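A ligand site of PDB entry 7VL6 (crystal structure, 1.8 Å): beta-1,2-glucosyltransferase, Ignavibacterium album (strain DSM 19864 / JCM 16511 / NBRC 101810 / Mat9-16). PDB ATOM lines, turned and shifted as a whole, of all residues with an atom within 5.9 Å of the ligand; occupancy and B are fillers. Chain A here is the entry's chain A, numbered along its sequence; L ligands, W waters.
The side-chain carboxylate of Glu 171 sits close to the side-chain carboxylate of Asp 304, 2.5 Å away. The backbone carbonyl oxygen (O) of Gln 101 sits at hydrogen-bond distance from the backbone NH (N) of Leu 95 (3.2 Å).
Water W3 lies within hydrogen-bond range of O2 of the ligand and NH2 of Arg 344. Water W4 lies within hydrogen-bond range of the backbone carbonyl oxygen of Asp 304 (2.7 Å), an oxygen (O5) of the ligand (2.8 Å), the backbone NH of Trp 274 (2.9 Å) and the backbone NH of Gly 273 (3.3 Å). Water W2 lies within hydrogen-bond range of OE1 of Glu 338 and O4 of the ligand. Water W1 lies within hydrogen-bond range of the side-chain carboxylate (OE2) of Glu 338, the side-chain amide nitrogen (ND2) of Asn 170, the side-chain carboxylate (OE2) of Glu 171 and an oxygen (O4) of the ligand.
An oxygen (O4) of the ligand is in hydrogen-bond range of the side-chain carboxylate of Glu 171 (2.6 Å). The backbone NH (N) of Trp 274 sits at hydrogen-bond distance from an oxygen (O6) of the ligand (3.3 Å). An oxygen (O7) of the ligand is in hydrogen-bond range of the backbone carbonyl oxygen (O) of Trp 274, 2.7 Å away. O7 of the ligand is in hydrogen-bond range of NH1 of Arg 344, 2.8 Å away. N of Gly 273 is in hydrogen-bond range of O6 of the ligand, at 2.9 Å. The side-chain hydroxyl (OH) of Tyr 387 is in hydrogen-bond range of an oxygen (O1) of the ligand (3.0 Å). NE2 of Gln 101 lies within hydrogen-bond range of O1 of the ligand (3.3 Å).
Leu 95 touches the ligand. Trp 177 touches the ligand (CZ3 to O6, 3.5 Å). CD1 of Leu 178 touches C3 of the ligand, at 3.4 Å. Pro 272 touches the ligand. CG1 of Ile 275 touches O7 of the ligand (3.6 Å). Ile 306 touches the ligand. Of the 21 residues printed, 12 come within 4 Å of the ligand.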
ATOM      1  N   LEU A  95      -5.532  -0.630 -22.672  1.00  0.00           N
ATOM      2  CA  LEU A  95      -4.953  -0.008 -21.457  1.00  0.00           C
ATOM      3  C   LEU A  95      -4.581  -1.150 -20.498  1.00  0.00           C
ATOM      4  O   LEU A  95      -3.570  -1.847 -20.809  1.00  0.00           O
ATOM      5  CB  LEU A  95      -5.930   1.020 -20.854  1.00  0.00           C
ATOM      6  CG  LEU A  95      -5.864   2.398 -21.527  1.00  0.00           C
ATOM      7  CD1 LEU A  95      -6.452   2.371 -22.951  1.00  0.00           C
ATOM      8  CD2 LEU A  95      -6.575   3.457 -20.666  1.00  0.00           C
ATOM      9  N   GLU A  97      -3.063  -1.729 -17.846  1.00  0.00           N
ATOM     10  CA  GLU A  97      -1.659  -1.850 -17.324  1.00  0.00           C
ATOM     11  C   GLU A  97      -0.932  -2.925 -18.101  1.00  0.00           C
ATOM     12  O   GLU A  97      -0.121  -3.644 -17.503  1.00  0.00           O
ATOM     13  CB  GLU A  97      -1.632  -2.262 -15.850  1.00  0.00           C
ATOM     14  CG  GLU A  97      -2.257  -1.233 -14.964  1.00  0.00           C
ATOM     15  CD  GLU A  97      -1.670  -1.208 -13.569  1.00  0.00           C
ATOM     16  OE1 GLU A  97      -1.140  -2.261 -13.114  1.00  0.00           O
ATOM     17  OE2 GLU A  97      -1.748  -0.148 -12.960  1.00  0.00           O
ATOM     18  N   GLN A 101      -0.155  -0.391 -23.846  1.00  0.00           N
ATOM     19  CA  GLN A 101      -1.648  -0.282 -23.765  1.00  0.00           C
ATOM     20  C   GLN A 101      -2.330  -1.380 -24.608  1.00  0.00           C
ATOM     21  O   GLN A 101      -3.499  -1.194 -25.026  1.00  0.00           O
ATOM     22  CB  GLN A 101      -2.050   1.143 -24.163  1.00  0.00           C
ATOM     23  CG  GLN A 101      -1.197   2.230 -23.500  1.00  0.00           C
ATOM     24  CD  GLN A 101      -1.425   2.307 -22.014  1.00  0.00           C
ATOM     25  OE1 GLN A 101      -2.131   1.492 -21.423  1.00  0.00           O
ATOM     26  NE2 GLN A 101      -0.779   3.247 -21.360  1.00  0.00           N
ATOM     27  N   ASN A 170     -11.190   1.111 -26.091  1.00  0.00           N
ATOM     28  CA  ASN A 170     -11.201   1.311 -24.611  1.00  0.00           C
ATOM     29  C   ASN A 170     -11.073   2.805 -24.315  1.00  0.00           C
ATOM     30  O   ASN A 170     -10.067   3.406 -24.715  1.00  0.00           O
ATOM     31  CB  ASN A 170     -10.097   0.496 -23.935  1.00  0.00           C
ATOM     32  CG  ASN A 170     -10.239   0.438 -22.426  1.00  0.00           C
ATOM     33  OD1 ASN A 170     -10.982  -0.400 -21.881  1.00  0.00           O
ATOM     34  ND2 ASN A 170      -9.655   1.408 -21.733  1.00  0.00           N
ATOM     35  N   GLU A 171     -12.067   3.386 -23.666  1.00  0.00           N
ATOM     36  CA  GLU A 171     -12.021   4.803 -23.183  1.00  0.00           C
ATOM     37  C   GLU A 171     -11.441   5.750 -24.249  1.00  0.00           C
ATOM     38  O   GLU A 171     -10.376   6.399 -24.010  1.00  0.00           O
ATOM     39  CB  GLU A 171     -11.191   4.839 -21.896  1.00  0.00           C
ATOM     40  CG  GLU A 171     -11.820   4.107 -20.711  1.00  0.00           C
ATOM     41  CD  GLU A 171     -11.033   4.232 -19.412  1.00  0.00           C
ATOM     42  OE1 GLU A 171      -9.837   4.516 -19.467  1.00  0.00           O
ATOM     43  OE2 GLU A 171     -11.663   4.101 -18.309  1.00  0.00           O
ATOM     44  N   VAL A 174      -8.828   8.766 -23.771  1.00  0.00           N
ATOM     45  CA  VAL A 174      -8.263   8.753 -22.387  1.00  0.00           C
ATOM     46  C   VAL A 174      -6.783   9.157 -22.437  1.00  0.00           C
ATOM     47  O   VAL A 174      -6.323   9.849 -21.531  1.00  0.00           O
ATOM     48  CB  VAL A 174      -8.473   7.420 -21.643  1.00  0.00           C
ATOM     49  CG1 VAL A 174      -7.674   6.256 -22.235  1.00  0.00           C
ATOM     50  CG2 VAL A 174      -8.154   7.576 -20.160  1.00  0.00           C
ATOM     51  N   PHE A 175      -6.057   8.777 -23.499  1.00  0.00           N
ATOM     52  CA  PHE A 175      -4.612   9.103 -23.635  1.00  0.00           C
ATOM     53  C   PHE A 175      -4.381  10.551 -23.953  1.00  0.00           C
ATOM     54  O   PHE A 175      -3.436  11.086 -23.360  1.00  0.00           O
ATOM     55  CB  PHE A 175      -3.963   8.362 -24.779  1.00  0.00           C
ATOM     56  CG  PHE A 175      -4.015   6.908 -24.514  1.00  0.00           C
ATOM     57  CD1 PHE A 175      -3.446   6.421 -23.346  1.00  0.00           C
ATOM     58  CD2 PHE A 175      -4.691   6.049 -25.356  1.00  0.00           C
ATOM     59  CE1 PHE A 175      -3.509   5.071 -23.072  1.00  0.00           C
ATOM     60  CE2 PHE A 175      -4.771   4.709 -25.067  1.00  0.00           C
ATOM     61  CZ  PHE A 175      -4.170   4.218 -23.929  1.00  0.00           C
ATOM     62  N   TRP A 177      -6.303  12.952 -23.051  1.00  0.00           N
ATOM     63  CA  TRP A 177      -6.580  13.568 -21.725  1.00  0.00           C
ATOM     64  C   TRP A 177      -5.387  13.392 -20.762  1.00  0.00           C
ATOM     65  O   TRP A 177      -4.916  14.422 -20.279  1.00  0.00           O
ATOM     66  CB  TRP A 177      -7.922  12.993 -21.199  1.00  0.00           C
ATOM     67  CG  TRP A 177      -8.293  13.416 -19.808  1.00  0.00           C
ATOM     68  CD1 TRP A 177      -8.456  14.682 -19.325  1.00  0.00           C
ATOM     69  CD2 TRP A 177      -8.572  12.516 -18.721  1.00  0.00           C
ATOM     70  NE1 TRP A 177      -8.815  14.615 -18.001  1.00  0.00           N
ATOM     71  CE2 TRP A 177      -8.917  13.313 -17.613  1.00  0.00           C
ATOM     72  CE3 TRP A 177      -8.586  11.119 -18.582  1.00  0.00           C
ATOM     73  CZ2 TRP A 177      -9.215  12.761 -16.359  1.00  0.00           C
ATOM     74  CZ3 TRP A 177      -8.921  10.585 -17.355  1.00  0.00           C
ATOM     75  CH2 TRP A 177      -9.218  11.386 -16.265  1.00  0.00           C
ATOM     76  N   LEU A 178      -4.878  12.189 -20.482  1.00  0.00           N
ATOM     77  CA  LEU A 178      -3.833  11.947 -19.443  1.00  0.00           C
ATOM     78  C   LEU A 178      -2.448  12.431 -19.903  1.00  0.00           C
ATOM     79  O   LEU A 178      -1.661  12.828 -19.015  1.00  0.00           O
ATOM     80  CB  LEU A 178      -3.773  10.464 -19.077  1.00  0.00           C
ATOM     81  CG  LEU A 178      -5.026   9.917 -18.416  1.00  0.00           C
ATOM     82  CD1 LEU A 178      -4.823   8.467 -18.075  1.00  0.00           C
ATOM     83  CD2 LEU A 178      -5.392  10.729 -17.173  1.00  0.00           C
ATOM     84  N   ILE A 271     -16.528   4.738 -20.101  1.00  0.00           N
ATOM     85  CA  ILE A 271     -16.269   6.180 -19.846  1.00  0.00           C
ATOM     86  C   ILE A 271     -15.235   6.371 -18.743  1.00  0.00           C
ATOM     87  O   ILE A 271     -15.520   6.014 -17.586  1.00  0.00           O
ATOM     88  CB  ILE A 271     -17.586   6.876 -19.445  1.00  0.00           C
ATOM     89  CG1 ILE A 271     -18.667   6.682 -20.502  1.00  0.00           C
ATOM     90  CG2 ILE A 271     -17.332   8.353 -19.192  1.00  0.00           C
ATOM     91  CD1 ILE A 271     -20.062   6.876 -19.950  1.00  0.00           C
ATOM     92  N   PRO A 272     -14.099   7.037 -19.056  1.00  0.00           N
ATOM     93  CA  PRO A 272     -13.082   7.389 -18.074  1.00  0.00           C
ATOM     94  C   PRO A 272     -13.453   8.678 -17.338  1.00  0.00           C
ATOM     95  O   PRO A 272     -14.414   9.364 -17.768  1.00  0.00           O
ATOM     96  CB  PRO A 272     -11.861   7.666 -18.981  1.00  0.00           C
ATOM     97  CG  PRO A 272     -12.464   8.285 -20.232  1.00  0.00           C
ATOM     98  CD  PRO A 272     -13.799   7.597 -20.395  1.00  0.00           C
ATOM     99  N   GLY A 273     -12.715   9.037 -16.276  1.00  0.00           N
ATOM    100  CA  GLY A 273     -12.792  10.392 -15.704  1.00  0.00           C
ATOM    101  C   GLY A 273     -12.524  10.455 -14.220  1.00  0.00           C
ATOM    102  O   GLY A 273     -12.355  11.574 -13.694  1.00  0.00           O
ATOM    103  N   TRP A 274     -12.557   9.339 -13.492  1.00  0.00           N
ATOM    104  CA  TRP A 274     -12.186   9.406 -12.057  1.00  0.00           C
ATOM    105  C   TRP A 274     -10.670   9.516 -11.988  1.00  0.00           C
ATOM    106  O   TRP A 274      -9.938   8.819 -12.749  1.00  0.00           O
ATOM    107  CB  TRP A 274     -12.692   8.198 -11.281  1.00  0.00           C
ATOM    108  CG  TRP A 274     -14.148   8.051 -11.025  1.00  0.00           C
ATOM    109  CD1 TRP A 274     -15.099   7.607 -11.907  1.00  0.00           C
ATOM    110  CD2 TRP A 274     -14.821   8.144  -9.753  1.00  0.00           C
ATOM    111  NE1 TRP A 274     -16.306   7.475 -11.292  1.00  0.00           N
ATOM    112  CE2 TRP A 274     -16.175   7.796  -9.955  1.00  0.00           C
ATOM    113  CE3 TRP A 274     -14.415   8.510  -8.471  1.00  0.00           C
ATOM    114  CZ2 TRP A 274     -17.124   7.776  -8.929  1.00  0.00           C
ATOM    115  CZ3 TRP A 274     -15.348   8.538  -7.456  1.00  0.00           C
ATOM    116  CH2 TRP A 274     -16.680   8.151  -7.679  1.00  0.00           C
ATOM    117  N   ILE A 275     -10.186  10.335 -11.054  1.00  0.00           N
ATOM    118  CA  ILE A 275      -8.750  10.344 -10.698  1.00  0.00           C
ATOM    119  C   ILE A 275      -8.662  10.828  -9.239  1.00  0.00           C
ATOM    120  O   ILE A 275      -9.434  11.724  -8.855  1.00  0.00           O
ATOM    121  CB  ILE A 275      -7.963  11.208 -11.694  1.00  0.00           C
ATOM    122  CG1 ILE A 275      -6.462  10.939 -11.618  1.00  0.00           C
ATOM    123  CG2 ILE A 275      -8.336  12.673 -11.550  1.00  0.00           C
ATOM    124  CD1 ILE A 275      -5.643  11.638 -12.714  1.00  0.00           C
ATOM    125  N   TYR A 276      -7.775  10.195  -8.481  1.00  0.00           N
ATOM    126  CA  TYR A 276      -7.538  10.474  -7.042  1.00  0.00           C
ATOM    127  C   TYR A 276      -8.831  10.342  -6.237  1.00  0.00           C
ATOM    128  O   TYR A 276      -8.968  10.980  -5.170  1.00  0.00           O
ATOM    129  CB  TYR A 276      -6.881  11.858  -6.887  1.00  0.00           C
ATOM    130  CG  TYR A 276      -5.726  12.102  -7.845  1.00  0.00           C
ATOM    131  CD1 TYR A 276      -4.700  11.175  -7.995  1.00  0.00           C
ATOM    132  CD2 TYR A 276      -5.654  13.268  -8.600  1.00  0.00           C
ATOM    133  CE1 TYR A 276      -3.660  11.373  -8.901  1.00  0.00           C
ATOM    134  CE2 TYR A 276      -4.604  13.485  -9.500  1.00  0.00           C
ATOM    135  CZ  TYR A 276      -3.616  12.531  -9.646  1.00  0.00           C
ATOM    136  OH  TYR A 276      -2.600  12.727 -10.537  1.00  0.00           O
ATOM    137  N   ASP A 304     -16.768   3.897 -15.763  1.00  0.00           N
ATOM    138  CA  ASP A 304     -15.596   3.288 -15.074  1.00  0.00           C
ATOM    139  C   ASP A 304     -15.439   3.984 -13.716  1.00  0.00           C
ATOM    140  O   ASP A 304     -14.884   5.067 -13.673  1.00  0.00           O
ATOM    141  CB  ASP A 304     -14.389   3.335 -16.004  1.00  0.00           C
ATOM    142  CG  ASP A 304     -14.559   2.525 -17.270  1.00  0.00           C
ATOM    143  OD1 ASP A 304     -15.471   1.687 -17.317  1.00  0.00           O
ATOM    144  OD2 ASP A 304     -13.796   2.764 -18.239  1.00  0.00           O
ATOM    145  N   ILE A 306     -13.992   4.540 -10.104  1.00  0.00           N
ATOM    146  CA  ILE A 306     -12.754   4.332  -9.306  1.00  0.00           C
ATOM    147  C   ILE A 306     -12.786   5.274  -8.083  1.00  0.00           C
ATOM    148  O   ILE A 306     -11.977   6.213  -7.999  1.00  0.00           O
ATOM    149  CB  ILE A 306     -11.481   4.513 -10.147  1.00  0.00           C
ATOM    150  CG1 ILE A 306     -11.579   3.925 -11.557  1.00  0.00           C
ATOM    151  CG2 ILE A 306     -10.322   3.916  -9.387  1.00  0.00           C
ATOM    152  CD1 ILE A 306     -10.357   4.241 -12.382  1.00  0.00           C
ATOM    153  N   GLU A 338     -16.708  -0.861 -15.544  1.00  0.00           N
ATOM    154  CA  GLU A 338     -15.607  -1.159 -14.604  1.00  0.00           C
ATOM    155  C   GLU A 338     -16.053  -0.601 -13.258  1.00  0.00           C
ATOM    156  O   GLU A 338     -16.283   0.629 -13.145  1.00  0.00           O
ATOM    157  CB  GLU A 338     -14.277  -0.566 -15.095  1.00  0.00           C
ATOM    158  CG  GLU A 338     -13.800  -1.069 -16.454  1.00  0.00           C
ATOM    159  CD  GLU A 338     -12.608  -0.289 -16.974  1.00  0.00           C
ATOM    160  OE1 GLU A 338     -11.946   0.382 -16.150  1.00  0.00           O
ATOM    161  OE2 GLU A 338     -12.388  -0.251 -18.203  1.00  0.00           O
ATOM    162  N   ARG A 344      -5.821  -0.937  -8.484  1.00  0.00           N
ATOM    163  CA  ARG A 344      -4.768  -0.977  -9.527  1.00  0.00           C
ATOM    164  C   ARG A 344      -3.405  -0.616  -8.943  1.00  0.00           C
ATOM    165  O   ARG A 344      -2.368  -0.976  -9.578  1.00  0.00           O
ATOM    166  CB  ARG A 344      -5.137  -0.024 -10.668  1.00  0.00           C
ATOM    167  CG  ARG A 344      -5.282   1.444 -10.261  1.00  0.00           C
ATOM    168  CD  ARG A 344      -5.870   2.328 -11.356  1.00  0.00           C
ATOM    169  NE  ARG A 344      -6.102   3.722 -10.947  1.00  0.00           N
ATOM    170  CZ  ARG A 344      -6.336   4.715 -11.808  1.00  0.00           C
ATOM    171  NH1 ARG A 344      -6.507   5.949 -11.366  1.00  0.00           N
ATOM    172  NH2 ARG A 344      -6.362   4.478 -13.106  1.00  0.00           N
ATOM    173  N   PHE A 386       2.800  -3.285 -17.500  1.00  0.00           N
ATOM    174  CA  PHE A 386       3.280  -1.906 -17.774  1.00  0.00           C
ATOM    175  C   PHE A 386       4.182  -1.442 -16.606  1.00  0.00           C
ATOM    176  O   PHE A 386       5.247  -0.824 -16.904  1.00  0.00           O
ATOM    177  CB  PHE A 386       2.075  -0.993 -17.980  1.00  0.00           C
ATOM    178  CG  PHE A 386       2.425   0.300 -18.674  1.00  0.00           C
ATOM    179  CD1 PHE A 386       3.039   1.326 -17.979  1.00  0.00           C
ATOM    180  CD2 PHE A 386       2.153   0.470 -20.021  1.00  0.00           C
ATOM    181  CE1 PHE A 386       3.405   2.501 -18.625  1.00  0.00           C
ATOM    182  CE2 PHE A 386       2.490   1.654 -20.658  1.00  0.00           C
ATOM    183  CZ  PHE A 386       3.119   2.664 -19.956  1.00  0.00           C
ATOM    184  N   TYR A 387       3.804  -1.748 -15.353  1.00  0.00           N
ATOM    185  CA  TYR A 387       4.270  -1.085 -14.098  1.00  0.00           C
ATOM    186  C   TYR A 387       4.818  -2.020 -13.004  1.00  0.00           C
ATOM    187  O   TYR A 387       5.183  -1.469 -11.914  1.00  0.00           O
ATOM    188  CB  TYR A 387       3.115  -0.363 -13.403  1.00  0.00           C
ATOM    189  CG  TYR A 387       2.599   0.855 -14.109  1.00  0.00           C
ATOM    190  CD1 TYR A 387       3.408   1.974 -14.269  1.00  0.00           C
ATOM    191  CD2 TYR A 387       1.290   0.913 -14.562  1.00  0.00           C
ATOM    192  CE1 TYR A 387       2.951   3.108 -14.925  1.00  0.00           C
ATOM    193  CE2 TYR A 387       0.817   2.039 -15.216  1.00  0.00           C
ATOM    194  CZ  TYR A 387       1.627   3.160 -15.348  1.00  0.00           C
ATOM    195  OH  TYR A 387       1.166   4.265 -15.988  1.00  0.00           O
HETATM  196  O1  LIG L   1      -0.798   4.369 -18.282  1.00  0.00           O
HETATM  197  C1  LIG L   1      -2.092   4.397 -17.776  1.00  0.00           C
HETATM  198  C2  LIG L   1      -3.126   5.167 -18.355  1.00  0.00           C
HETATM  199  C3  LIG L   1      -4.454   5.134 -17.844  1.00  0.00           C
HETATM  200  C4  LIG L   1      -2.428   3.620 -16.657  1.00  0.00           C
HETATM  201  C5  LIG L   1      -3.731   3.631 -16.129  1.00  0.00           C
HETATM  202  C6  LIG L   1      -4.771   4.388 -16.706  1.00  0.00           C
HETATM  203  O2  LIG L   1      -6.044   4.287 -16.160  1.00  0.00           O
HETATM  204  C7  LIG L   1      -7.111   5.244 -16.385  1.00  0.00           C
HETATM  205  O3  LIG L   1      -6.931   6.252 -15.385  1.00  0.00           O
HETATM  206  C8  LIG L   1      -8.506   4.657 -16.231  1.00  0.00           C
HETATM  207  O4  LIG L   1      -8.816   3.663 -17.244  1.00  0.00           O
HETATM  208  C9  LIG L   1      -9.579   5.798 -16.238  1.00  0.00           C
HETATM  209  O5  LIG L   1     -10.857   5.270 -15.980  1.00  0.00           O
HETATM  210  C10 LIG L   1      -9.233   6.896 -15.211  1.00  0.00           C
HETATM  211  O6  LIG L   1     -10.149   7.997 -15.332  1.00  0.00           O
HETATM  212  C11 LIG L   1      -7.822   7.374 -15.481  1.00  0.00           C
HETATM  213  C12 LIG L   1      -7.265   8.402 -14.477  1.00  0.00           C
HETATM  214  O7  LIG L   1      -7.458   7.849 -13.131  1.00  0.00           O
HETATM  215  O   HOH W   1     -10.449   1.521 -18.965  1.00  0.00           O
HETATM  216  O   HOH W   2      -9.327   1.398 -15.524  1.00  0.00           O
HETATM  217  O   HOH W   3      -6.005   1.972 -14.607  1.00  0.00           O
HETATM  218  O   HOH W   4     -12.658   6.496 -14.229  1.00  0.00           O
